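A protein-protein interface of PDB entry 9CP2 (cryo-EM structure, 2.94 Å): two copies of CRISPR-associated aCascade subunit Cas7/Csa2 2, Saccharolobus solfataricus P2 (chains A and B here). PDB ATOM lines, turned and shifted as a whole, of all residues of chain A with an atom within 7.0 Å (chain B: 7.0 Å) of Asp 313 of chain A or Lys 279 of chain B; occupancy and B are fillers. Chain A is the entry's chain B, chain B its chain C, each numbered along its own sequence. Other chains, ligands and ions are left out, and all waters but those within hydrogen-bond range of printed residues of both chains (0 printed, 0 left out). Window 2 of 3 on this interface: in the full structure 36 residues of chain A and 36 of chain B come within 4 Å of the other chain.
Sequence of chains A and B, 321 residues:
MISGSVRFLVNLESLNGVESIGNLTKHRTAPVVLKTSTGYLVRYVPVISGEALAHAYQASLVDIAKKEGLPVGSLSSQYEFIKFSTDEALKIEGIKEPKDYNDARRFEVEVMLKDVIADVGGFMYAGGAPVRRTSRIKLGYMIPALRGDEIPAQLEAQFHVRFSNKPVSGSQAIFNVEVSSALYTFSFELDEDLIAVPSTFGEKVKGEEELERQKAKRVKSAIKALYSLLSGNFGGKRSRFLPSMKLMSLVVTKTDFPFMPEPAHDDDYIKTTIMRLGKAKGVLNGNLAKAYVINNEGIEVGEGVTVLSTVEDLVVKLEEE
OE2 of Glu 312 of chain A lies within salt-bridge range of NE of Arg 276 of chain B, at 3.8 Å.
The side-chain carboxylate (OE2) of Glu 312 of chain A sits at hydrogen-bond distance from the side-chain hydroxyl (OH) of Tyr 227 of chain A (3.0 Å).
OG1 of Thr 310 of chain A is in hydrogen-bond range of OE1 of Glu 312 of chain A (2.6 Å).
The side-chain hydroxyl (OG1) of Thr 310 of chain A lies within hydrogen-bond range of the side-chain carboxylate (OD2) of Asp 313 of chain A (3.3 Å).
Among the printed residues, pairs that only touch across the chains: Asp 313 of chain A with Lys 279 of chain B (3.3 Å), Val 315 of chain A with Val 283 of chain B (3.9 Å) and Tyr 227 of chain A with Leu 284 of chain B (3.95 Å).
Ser 309 of chain A touches none of the printed residues of chain B.
Of the printed residues of chain B, Glu 312 of chain A touches Arg 276 (3.6 Å).
Asp 313 of chain A touches just one residue of chain B: Lys 279 (3.3 Å).
Of the printed residues of chain A, Arg 276 of chain B touches Glu 312.
No residue of chain A comes within 4 Å of Gly 278 of chain B.
The nearest residue of chain B that does not touch Asp 313 of chain A is Val 283 of chain B (6.5 Å).
The nearest printed residue of chain A that does not touch Lys 279 of chain B is Glu 312 of chain A (4.02 Å).
The nearest printed residue of chain A that does not touch Arg 276 of chain B is Thr 310 of chain A (4.2 Å).
Hydrophobic or aromatic side chains of chain B within 4 Å of the printed part of chain A: Val 283 and Leu 284.
Of the 13 printed residues of chain A, 4 touch a printed residue of chain B.
Printed residues of chain A that touch a printed residue of chain B: Tyr 227, Glu 312, Asp 313 and Val 315.
Along chain A the printed residues that touch a printed residue of chain B span positions 227 to 315.
Among the printed residues, 4 pairs touch across the chains.
No position is printed for both chains.
Of the 4 pairs that touch across the chains among the printed residues, none has its exchanged pair printed and touching as well.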
ATOM      1  N   TYR A 227     -38.449   9.912   3.609  1.00  0.00           N
ATOM      2  CA  TYR A 227     -37.533   8.782   3.708  1.00  0.00           C
ATOM      3  C   TYR A 227     -38.145   7.640   4.504  1.00  0.00           C
ATOM      4  O   TYR A 227     -37.922   6.466   4.188  1.00  0.00           O
ATOM      5  CB  TYR A 227     -36.215   9.229   4.336  1.00  0.00           C
ATOM      6  CG  TYR A 227     -35.196   8.123   4.414  1.00  0.00           C
ATOM      7  CD1 TYR A 227     -34.842   7.399   3.286  1.00  0.00           C
ATOM      8  CD2 TYR A 227     -34.594   7.794   5.619  1.00  0.00           C
ATOM      9  CE1 TYR A 227     -33.914   6.381   3.353  1.00  0.00           C
ATOM     10  CE2 TYR A 227     -33.663   6.777   5.696  1.00  0.00           C
ATOM     11  CZ  TYR A 227     -33.327   6.073   4.560  1.00  0.00           C
ATOM     12  OH  TYR A 227     -32.402   5.058   4.626  1.00  0.00           O
ATOM     13  N   LEU A 308     -31.465   5.688 -10.794  1.00  0.00           N
ATOM     14  CA  LEU A 308     -30.839   5.763  -9.485  1.00  0.00           C
ATOM     15  C   LEU A 308     -30.568   4.361  -8.948  1.00  0.00           C
ATOM     16  O   LEU A 308     -30.744   3.354  -9.637  1.00  0.00           O
ATOM     17  CB  LEU A 308     -31.714   6.564  -8.519  1.00  0.00           C
ATOM     18  CG  LEU A 308     -31.975   8.018  -8.906  1.00  0.00           C
ATOM     19  CD1 LEU A 308     -33.070   8.605  -8.034  1.00  0.00           C
ATOM     20  CD2 LEU A 308     -30.701   8.835  -8.796  1.00  0.00           C
ATOM     21  N   SER A 309     -30.118   4.300  -7.702  1.00  0.00           N
ATOM     22  CA  SER A 309     -29.817   3.025  -7.058  1.00  0.00           C
ATOM     23  C   SER A 309     -30.528   2.841  -5.725  1.00  0.00           C
ATOM     24  O   SER A 309     -30.917   1.719  -5.397  1.00  0.00           O
ATOM     25  CB  SER A 309     -28.303   2.888  -6.857  1.00  0.00           C
ATOM     26  OG  SER A 309     -27.628   2.850  -8.100  1.00  0.00           O
ATOM     27  N   THR A 310     -30.700   3.909  -4.947  1.00  0.00           N
ATOM     28  CA  THR A 310     -31.308   3.811  -3.624  1.00  0.00           C
ATOM     29  C   THR A 310     -32.330   4.920  -3.422  1.00  0.00           C
ATOM     30  O   THR A 310     -32.704   5.610  -4.375  1.00  0.00           O
ATOM     31  CB  THR A 310     -30.259   3.884  -2.511  1.00  0.00           C
ATOM     32  OG1 THR A 310     -29.853   5.245  -2.324  1.00  0.00           O
ATOM     33  CG2 THR A 310     -29.042   3.028  -2.827  1.00  0.00           C
ATOM     34  N   VAL A 311     -32.787   5.094  -2.184  1.00  0.00           N
ATOM     35  CA  VAL A 311     -33.803   6.091  -1.866  1.00  0.00           C
ATOM     36  C   VAL A 311     -33.142   7.356  -1.335  1.00  0.00           C
ATOM     37  O   VAL A 311     -33.629   8.469  -1.567  1.00  0.00           O
ATOM     38  CB  VAL A 311     -34.817   5.536  -0.852  1.00  0.00           C
ATOM     39  CG1 VAL A 311     -35.939   6.525  -0.637  1.00  0.00           C
ATOM     40  CG2 VAL A 311     -35.356   4.200  -1.329  1.00  0.00           C
ATOM     41  N   GLU A 312     -32.026   7.196  -0.619  1.00  0.00           N
ATOM     42  CA  GLU A 312     -31.301   8.356  -0.113  1.00  0.00           C
ATOM     43  C   GLU A 312     -30.815   9.236  -1.258  1.00  0.00           C
ATOM     44  O   GLU A 312     -30.806  10.470  -1.145  1.00  0.00           O
ATOM     45  CB  GLU A 312     -30.131   7.898   0.756  1.00  0.00           C
ATOM     46  CG  GLU A 312     -30.536   6.935   1.859  1.00  0.00           C
ATOM     47  CD  GLU A 312     -30.353   5.484   1.460  1.00  0.00           C
ATOM     48  OE1 GLU A 312     -29.960   5.234   0.305  1.00  0.00           O
ATOM     49  OE2 GLU A 312     -30.608   4.593   2.297  1.00  0.00           O
ATOM     50  N   ASP A 313     -30.415   8.618  -2.371  1.00  0.00           N
ATOM     51  CA  ASP A 313     -30.061   9.385  -3.558  1.00  0.00           C
ATOM     52  C   ASP A 313     -31.242  10.211  -4.044  1.00  0.00           C
ATOM     53  O   ASP A 313     -31.088  11.387  -4.396  1.00  0.00           O
ATOM     54  CB  ASP A 313     -29.582   8.442  -4.660  1.00  0.00           C
ATOM     55  CG  ASP A 313     -28.312   7.717  -4.289  1.00  0.00           C
ATOM     56  OD1 ASP A 313     -27.538   8.261  -3.474  1.00  0.00           O
ATOM     57  OD2 ASP A 313     -28.085   6.605  -4.809  1.00  0.00           O
ATOM     58  N   LEU A 314     -32.432   9.609  -4.070  1.00  0.00           N
ATOM     59  CA  LEU A 314     -33.619  10.342  -4.492  1.00  0.00           C
ATOM     60  C   LEU A 314     -33.916  11.494  -3.546  1.00  0.00           C
ATOM     61  O   LEU A 314     -34.309  12.579  -3.987  1.00  0.00           O
ATOM     62  CB  LEU A 314     -34.817   9.399  -4.581  1.00  0.00           C
ATOM     63  CG  LEU A 314     -36.113  10.041  -5.078  1.00  0.00           C
ATOM     64  CD1 LEU A 314     -35.942  10.552  -6.497  1.00  0.00           C
ATOM     65  CD2 LEU A 314     -37.269   9.064  -4.991  1.00  0.00           C
ATOM     66  N   VAL A 315     -33.734  11.282  -2.241  1.00  0.00           N
ATOM     67  CA  VAL A 315     -33.980  12.347  -1.271  1.00  0.00           C
ATOM     68  C   VAL A 315     -33.013  13.503  -1.490  1.00  0.00           C
ATOM     69  O   VAL A 315     -33.408  14.676  -1.473  1.00  0.00           O
ATOM     70  CB  VAL A 315     -33.890  11.793   0.162  1.00  0.00           C
ATOM     71  CG1 VAL A 315     -34.009  12.919   1.174  1.00  0.00           C
ATOM     72  CG2 VAL A 315     -34.972  10.753   0.395  1.00  0.00           C
ATOM     73  N   VAL A 316     -31.733  13.193  -1.712  1.00  0.00           N
ATOM     74  CA  VAL A 316     -30.747  14.243  -1.954  1.00  0.00           C
ATOM     75  C   VAL A 316     -31.077  15.007  -3.230  1.00  0.00           C
ATOM     76  O   VAL A 316     -31.028  16.244  -3.263  1.00  0.00           O
ATOM     77  CB  VAL A 316     -29.330  13.641  -2.004  1.00  0.00           C
ATOM     78  CG1 VAL A 316     -28.339  14.654  -2.553  1.00  0.00           C
ATOM     79  CG2 VAL A 316     -28.909  13.170  -0.625  1.00  0.00           C
ATOM     80  N   LYS A 317     -31.425  14.286  -4.300  1.00  0.00           N
ATOM     81  CA  LYS A 317     -31.738  14.944  -5.565  1.00  0.00           C
ATOM     82  C   LYS A 317     -32.981  15.817  -5.440  1.00  0.00           C
ATOM     83  O   LYS A 317     -33.039  16.911  -6.012  1.00  0.00           O
ATOM     84  CB  LYS A 317     -31.916  13.901  -6.667  1.00  0.00           C
ATOM     85  CG  LYS A 317     -30.633  13.169  -7.018  1.00  0.00           C
ATOM     86  CD  LYS A 317     -30.446  13.046  -8.516  1.00  0.00           C
ATOM     87  CE  LYS A 317     -29.121  12.375  -8.843  1.00  0.00           C
ATOM     88  NZ  LYS A 317     -28.859  12.343 -10.307  1.00  0.00           N
ATOM     89  N   LEU A 318     -33.987  15.346  -4.703  1.00  0.00           N
ATOM     90  CA  LEU A 318     -35.173  16.160  -4.458  1.00  0.00           C
ATOM     91  C   LEU A 318     -34.827  17.412  -3.667  1.00  0.00           C
ATOM     92  O   LEU A 318     -35.360  18.494  -3.941  1.00  0.00           O
ATOM     93  CB  LEU A 318     -36.226  15.336  -3.718  1.00  0.00           C
ATOM     94  CG  LEU A 318     -37.009  14.317  -4.543  1.00  0.00           C
ATOM     95  CD1 LEU A 318     -37.588  13.235  -3.647  1.00  0.00           C
ATOM     96  CD2 LEU A 318     -38.108  15.010  -5.321  1.00  0.00           C
ATOM     97  N   GLU A 319     -33.948  17.285  -2.670  1.00  0.00           N
ATOM     98  CA  GLU A 319     -33.549  18.449  -1.886  1.00  0.00           C
ATOM     99  C   GLU A 319     -32.809  19.468  -2.742  1.00  0.00           C
ATOM    100  O   GLU A 319     -33.017  20.678  -2.597  1.00  0.00           O
ATOM    101  CB  GLU A 319     -32.676  18.021  -0.708  1.00  0.00           C
ATOM    102  CG  GLU A 319     -33.430  17.396   0.450  1.00  0.00           C
ATOM    103  CD  GLU A 319     -32.508  17.007   1.587  1.00  0.00           C
ATOM    104  OE1 GLU A 319     -31.579  17.785   1.891  1.00  0.00           O
ATOM    105  OE2 GLU A 319     -32.700  15.920   2.168  1.00  0.00           O
ATOM    106  N   PHE B 257     -29.164   6.774  14.470  1.00  0.00           N
ATOM    107  CA  PHE B 257     -30.363   7.143  13.737  1.00  0.00           C
ATOM    108  C   PHE B 257     -31.129   5.892  13.337  1.00  0.00           C
ATOM    109  O   PHE B 257     -30.545   4.806  13.248  1.00  0.00           O
ATOM    110  CB  PHE B 257     -30.016   7.959  12.481  1.00  0.00           C
ATOM    111  CG  PHE B 257     -28.900   7.372  11.666  1.00  0.00           C
ATOM    112  CD1 PHE B 257     -29.166   6.450  10.669  1.00  0.00           C
ATOM    113  CD2 PHE B 257     -27.588   7.742  11.893  1.00  0.00           C
ATOM    114  CE1 PHE B 257     -28.146   5.907   9.920  1.00  0.00           C
ATOM    115  CE2 PHE B 257     -26.563   7.202  11.146  1.00  0.00           C
ATOM    116  CZ  PHE B 257     -26.843   6.283  10.159  1.00  0.00           C
ATOM    117  N   THR B 273     -26.509  -2.884   2.148  1.00  0.00           N
ATOM    118  CA  THR B 273     -26.787  -2.209   3.411  1.00  0.00           C
ATOM    119  C   THR B 273     -25.611  -1.348   3.855  1.00  0.00           C
ATOM    120  O   THR B 273     -25.822  -0.300   4.470  1.00  0.00           O
ATOM    121  CB  THR B 273     -27.167  -3.214   4.505  1.00  0.00           C
ATOM    122  OG1 THR B 273     -27.507  -2.502   5.702  1.00  0.00           O
ATOM    123  CG2 THR B 273     -26.029  -4.163   4.807  1.00  0.00           C
ATOM    124  N   ILE B 274     -24.378  -1.742   3.529  1.00  0.00           N
ATOM    125  CA  ILE B 274     -23.233  -0.886   3.831  1.00  0.00           C
ATOM    126  C   ILE B 274     -23.327   0.421   3.052  1.00  0.00           C
ATOM    127  O   ILE B 274     -23.117   1.511   3.601  1.00  0.00           O
ATOM    128  CB  ILE B 274     -21.916  -1.624   3.539  1.00  0.00           C
ATOM    129  CG1 ILE B 274     -21.590  -2.599   4.667  1.00  0.00           C
ATOM    130  CG2 ILE B 274     -20.778  -0.633   3.355  1.00  0.00           C
ATOM    131  CD1 ILE B 274     -20.834  -3.818   4.210  1.00  0.00           C
ATOM    132  N   MET B 275     -23.643   0.331   1.757  1.00  0.00           N
ATOM    133  CA  MET B 275     -23.774   1.538   0.946  1.00  0.00           C
ATOM    134  C   MET B 275     -24.916   2.415   1.444  1.00  0.00           C
ATOM    135  O   MET B 275     -24.776   3.644   1.548  1.00  0.00           O
ATOM    136  CB  MET B 275     -23.991   1.159  -0.519  1.00  0.00           C
ATOM    137  CG  MET B 275     -22.817   0.433  -1.149  1.00  0.00           C
ATOM    138  SD  MET B 275     -21.348   1.464  -1.310  1.00  0.00           S
ATOM    139  CE  MET B 275     -21.807   2.489  -2.705  1.00  0.00           C
ATOM    140  N   ARG B 276     -26.056   1.798   1.758  1.00  0.00           N
ATOM    141  CA  ARG B 276     -27.189   2.558   2.269  1.00  0.00           C
ATOM    142  C   ARG B 276     -26.855   3.214   3.597  1.00  0.00           C
ATOM    143  O   ARG B 276     -27.312   4.324   3.874  1.00  0.00           O
ATOM    144  CB  ARG B 276     -28.413   1.654   2.407  1.00  0.00           C
ATOM    145  CG  ARG B 276     -29.223   1.514   1.130  1.00  0.00           C
ATOM    146  CD  ARG B 276     -30.322   0.483   1.295  1.00  0.00           C
ATOM    147  NE  ARG B 276     -31.284   0.878   2.314  1.00  0.00           N
ATOM    148  CZ  ARG B 276     -31.593   0.141   3.372  1.00  0.00           C
ATOM    149  NH1 ARG B 276     -31.024  -1.032   3.586  1.00  0.00           N
ATOM    150  NH2 ARG B 276     -32.494   0.598   4.239  1.00  0.00           N
ATOM    151  N   LEU B 277     -26.059   2.547   4.435  1.00  0.00           N
ATOM    152  CA  LEU B 277     -25.643   3.149   5.698  1.00  0.00           C
ATOM    153  C   LEU B 277     -24.735   4.346   5.463  1.00  0.00           C
ATOM    154  O   LEU B 277     -24.896   5.396   6.099  1.00  0.00           O
ATOM    155  CB  LEU B 277     -24.938   2.106   6.561  1.00  0.00           C
ATOM    156  CG  LEU B 277     -24.318   2.641   7.848  1.00  0.00           C
ATOM    157  CD1 LEU B 277     -25.407   2.984   8.838  1.00  0.00           C
ATOM    158  CD2 LEU B 277     -23.351   1.629   8.432  1.00  0.00           C
ATOM    159  N   GLY B 278     -23.775   4.203   4.548  1.00  0.00           N
ATOM    160  CA  GLY B 278     -22.895   5.313   4.235  1.00  0.00           C
ATOM    161  C   GLY B 278     -23.651   6.528   3.738  1.00  0.00           C
ATOM    162  O   GLY B 278     -23.329   7.662   4.095  1.00  0.00           O
ATOM    163  N   LYS B 279     -24.673   6.307   2.908  1.00  0.00           N
ATOM    164  CA  LYS B 279     -25.461   7.434   2.416  1.00  0.00           C
ATOM    165  C   LYS B 279     -26.417   7.977   3.478  1.00  0.00           C
ATOM    166  O   LYS B 279     -26.601   9.198   3.584  1.00  0.00           O
ATOM    167  CB  LYS B 279     -26.227   7.018   1.163  1.00  0.00           C
ATOM    168  CG  LYS B 279     -25.324   6.700  -0.012  1.00  0.00           C
ATOM    169  CD  LYS B 279     -26.122   6.307  -1.237  1.00  0.00           C
ATOM    170  CE  LYS B 279     -25.213   6.078  -2.431  1.00  0.00           C
ATOM    171  NZ  LYS B 279     -24.335   4.890  -2.237  1.00  0.00           N
ATOM    172  N   ALA B 280     -27.025   7.093   4.274  1.00  0.00           N
ATOM    173  CA  ALA B 280     -28.014   7.509   5.257  1.00  0.00           C
ATOM    174  C   ALA B 280     -27.382   8.285   6.399  1.00  0.00           C
ATOM    175  O   ALA B 280     -28.039   9.144   6.998  1.00  0.00           O
ATOM    176  CB  ALA B 280     -28.763   6.291   5.795  1.00  0.00           C
ATOM    177  N   LYS B 281     -26.122   7.990   6.726  1.00  0.00           N
ATOM    178  CA  LYS B 281     -25.430   8.786   7.733  1.00  0.00           C
ATOM    179  C   LYS B 281     -25.362  10.246   7.310  1.00  0.00           C
ATOM    180  O   LYS B 281     -25.602  11.149   8.121  1.00  0.00           O
ATOM    181  CB  LYS B 281     -24.029   8.229   7.974  1.00  0.00           C
ATOM    182  CG  LYS B 281     -23.224   9.006   8.997  1.00  0.00           C
ATOM    183  CD  LYS B 281     -21.832   8.426   9.157  1.00  0.00           C
ATOM    184  CE  LYS B 281     -21.014   9.238  10.143  1.00  0.00           C
ATOM    185  NZ  LYS B 281     -19.745   8.549  10.503  1.00  0.00           N
ATOM    186  N   GLY B 282     -25.042  10.495   6.040  1.00  0.00           N
ATOM    187  CA  GLY B 282     -24.995  11.865   5.558  1.00  0.00           C
ATOM    188  C   GLY B 282     -26.369  12.498   5.440  1.00  0.00           C
ATOM    189  O   GLY B 282     -26.573  13.642   5.858  1.00  0.00           O
ATOM    190  N   VAL B 283     -27.334  11.765   4.875  1.00  0.00           N
ATOM    191  CA  VAL B 283     -28.619  12.388   4.562  1.00  0.00           C
ATOM    192  C   VAL B 283     -29.397  12.734   5.830  1.00  0.00           C
ATOM    193  O   VAL B 283     -30.160  13.707   5.849  1.00  0.00           O
ATOM    194  CB  VAL B 283     -29.447  11.494   3.615  1.00  0.00           C
ATOM    195  CG1 VAL B 283     -29.966  10.265   4.334  1.00  0.00           C
ATOM    196  CG2 VAL B 283     -30.595  12.282   3.005  1.00  0.00           C
ATOM    197  N   LEU B 284     -29.228  11.961   6.901  1.00  0.00           N
ATOM    198  CA  LEU B 284     -29.968  12.177   8.138  1.00  0.00           C
ATOM    199  C   LEU B 284     -29.179  12.953   9.183  1.00  0.00           C
ATOM    200  O   LEU B 284     -29.650  13.088  10.318  1.00  0.00           O
ATOM    201  CB  LEU B 284     -30.423  10.841   8.726  1.00  0.00           C
ATOM    202  CG  LEU B 284     -31.448  10.054   7.912  1.00  0.00           C
ATOM    203  CD1 LEU B 284     -31.700   8.697   8.539  1.00  0.00           C
ATOM    204  CD2 LEU B 284     -32.742  10.842   7.808  1.00  0.00           C
ATOM    205  N   ASN B 285     -27.994  13.456   8.831  1.00  0.00           N
ATOM    206  CA  ASN B 285     -27.155  14.229   9.749  1.00  0.00           C
ATOM    207  C   ASN B 285     -26.787  13.404  10.981  1.00  0.00           C
ATOM    208  O   ASN B 285     -26.945  13.840  12.122  1.00  0.00           O
ATOM    209  CB  ASN B 285     -27.836  15.540  10.150  1.00  0.00           C
ATOM    210  CG  ASN B 285     -27.777  16.583   9.058  1.00  0.00           C
ATOM    211  OD1 ASN B 285     -26.764  16.725   8.373  1.00  0.00           O
ATOM    212  ND2 ASN B 285     -28.867  17.321   8.884  1.00  0.00           N
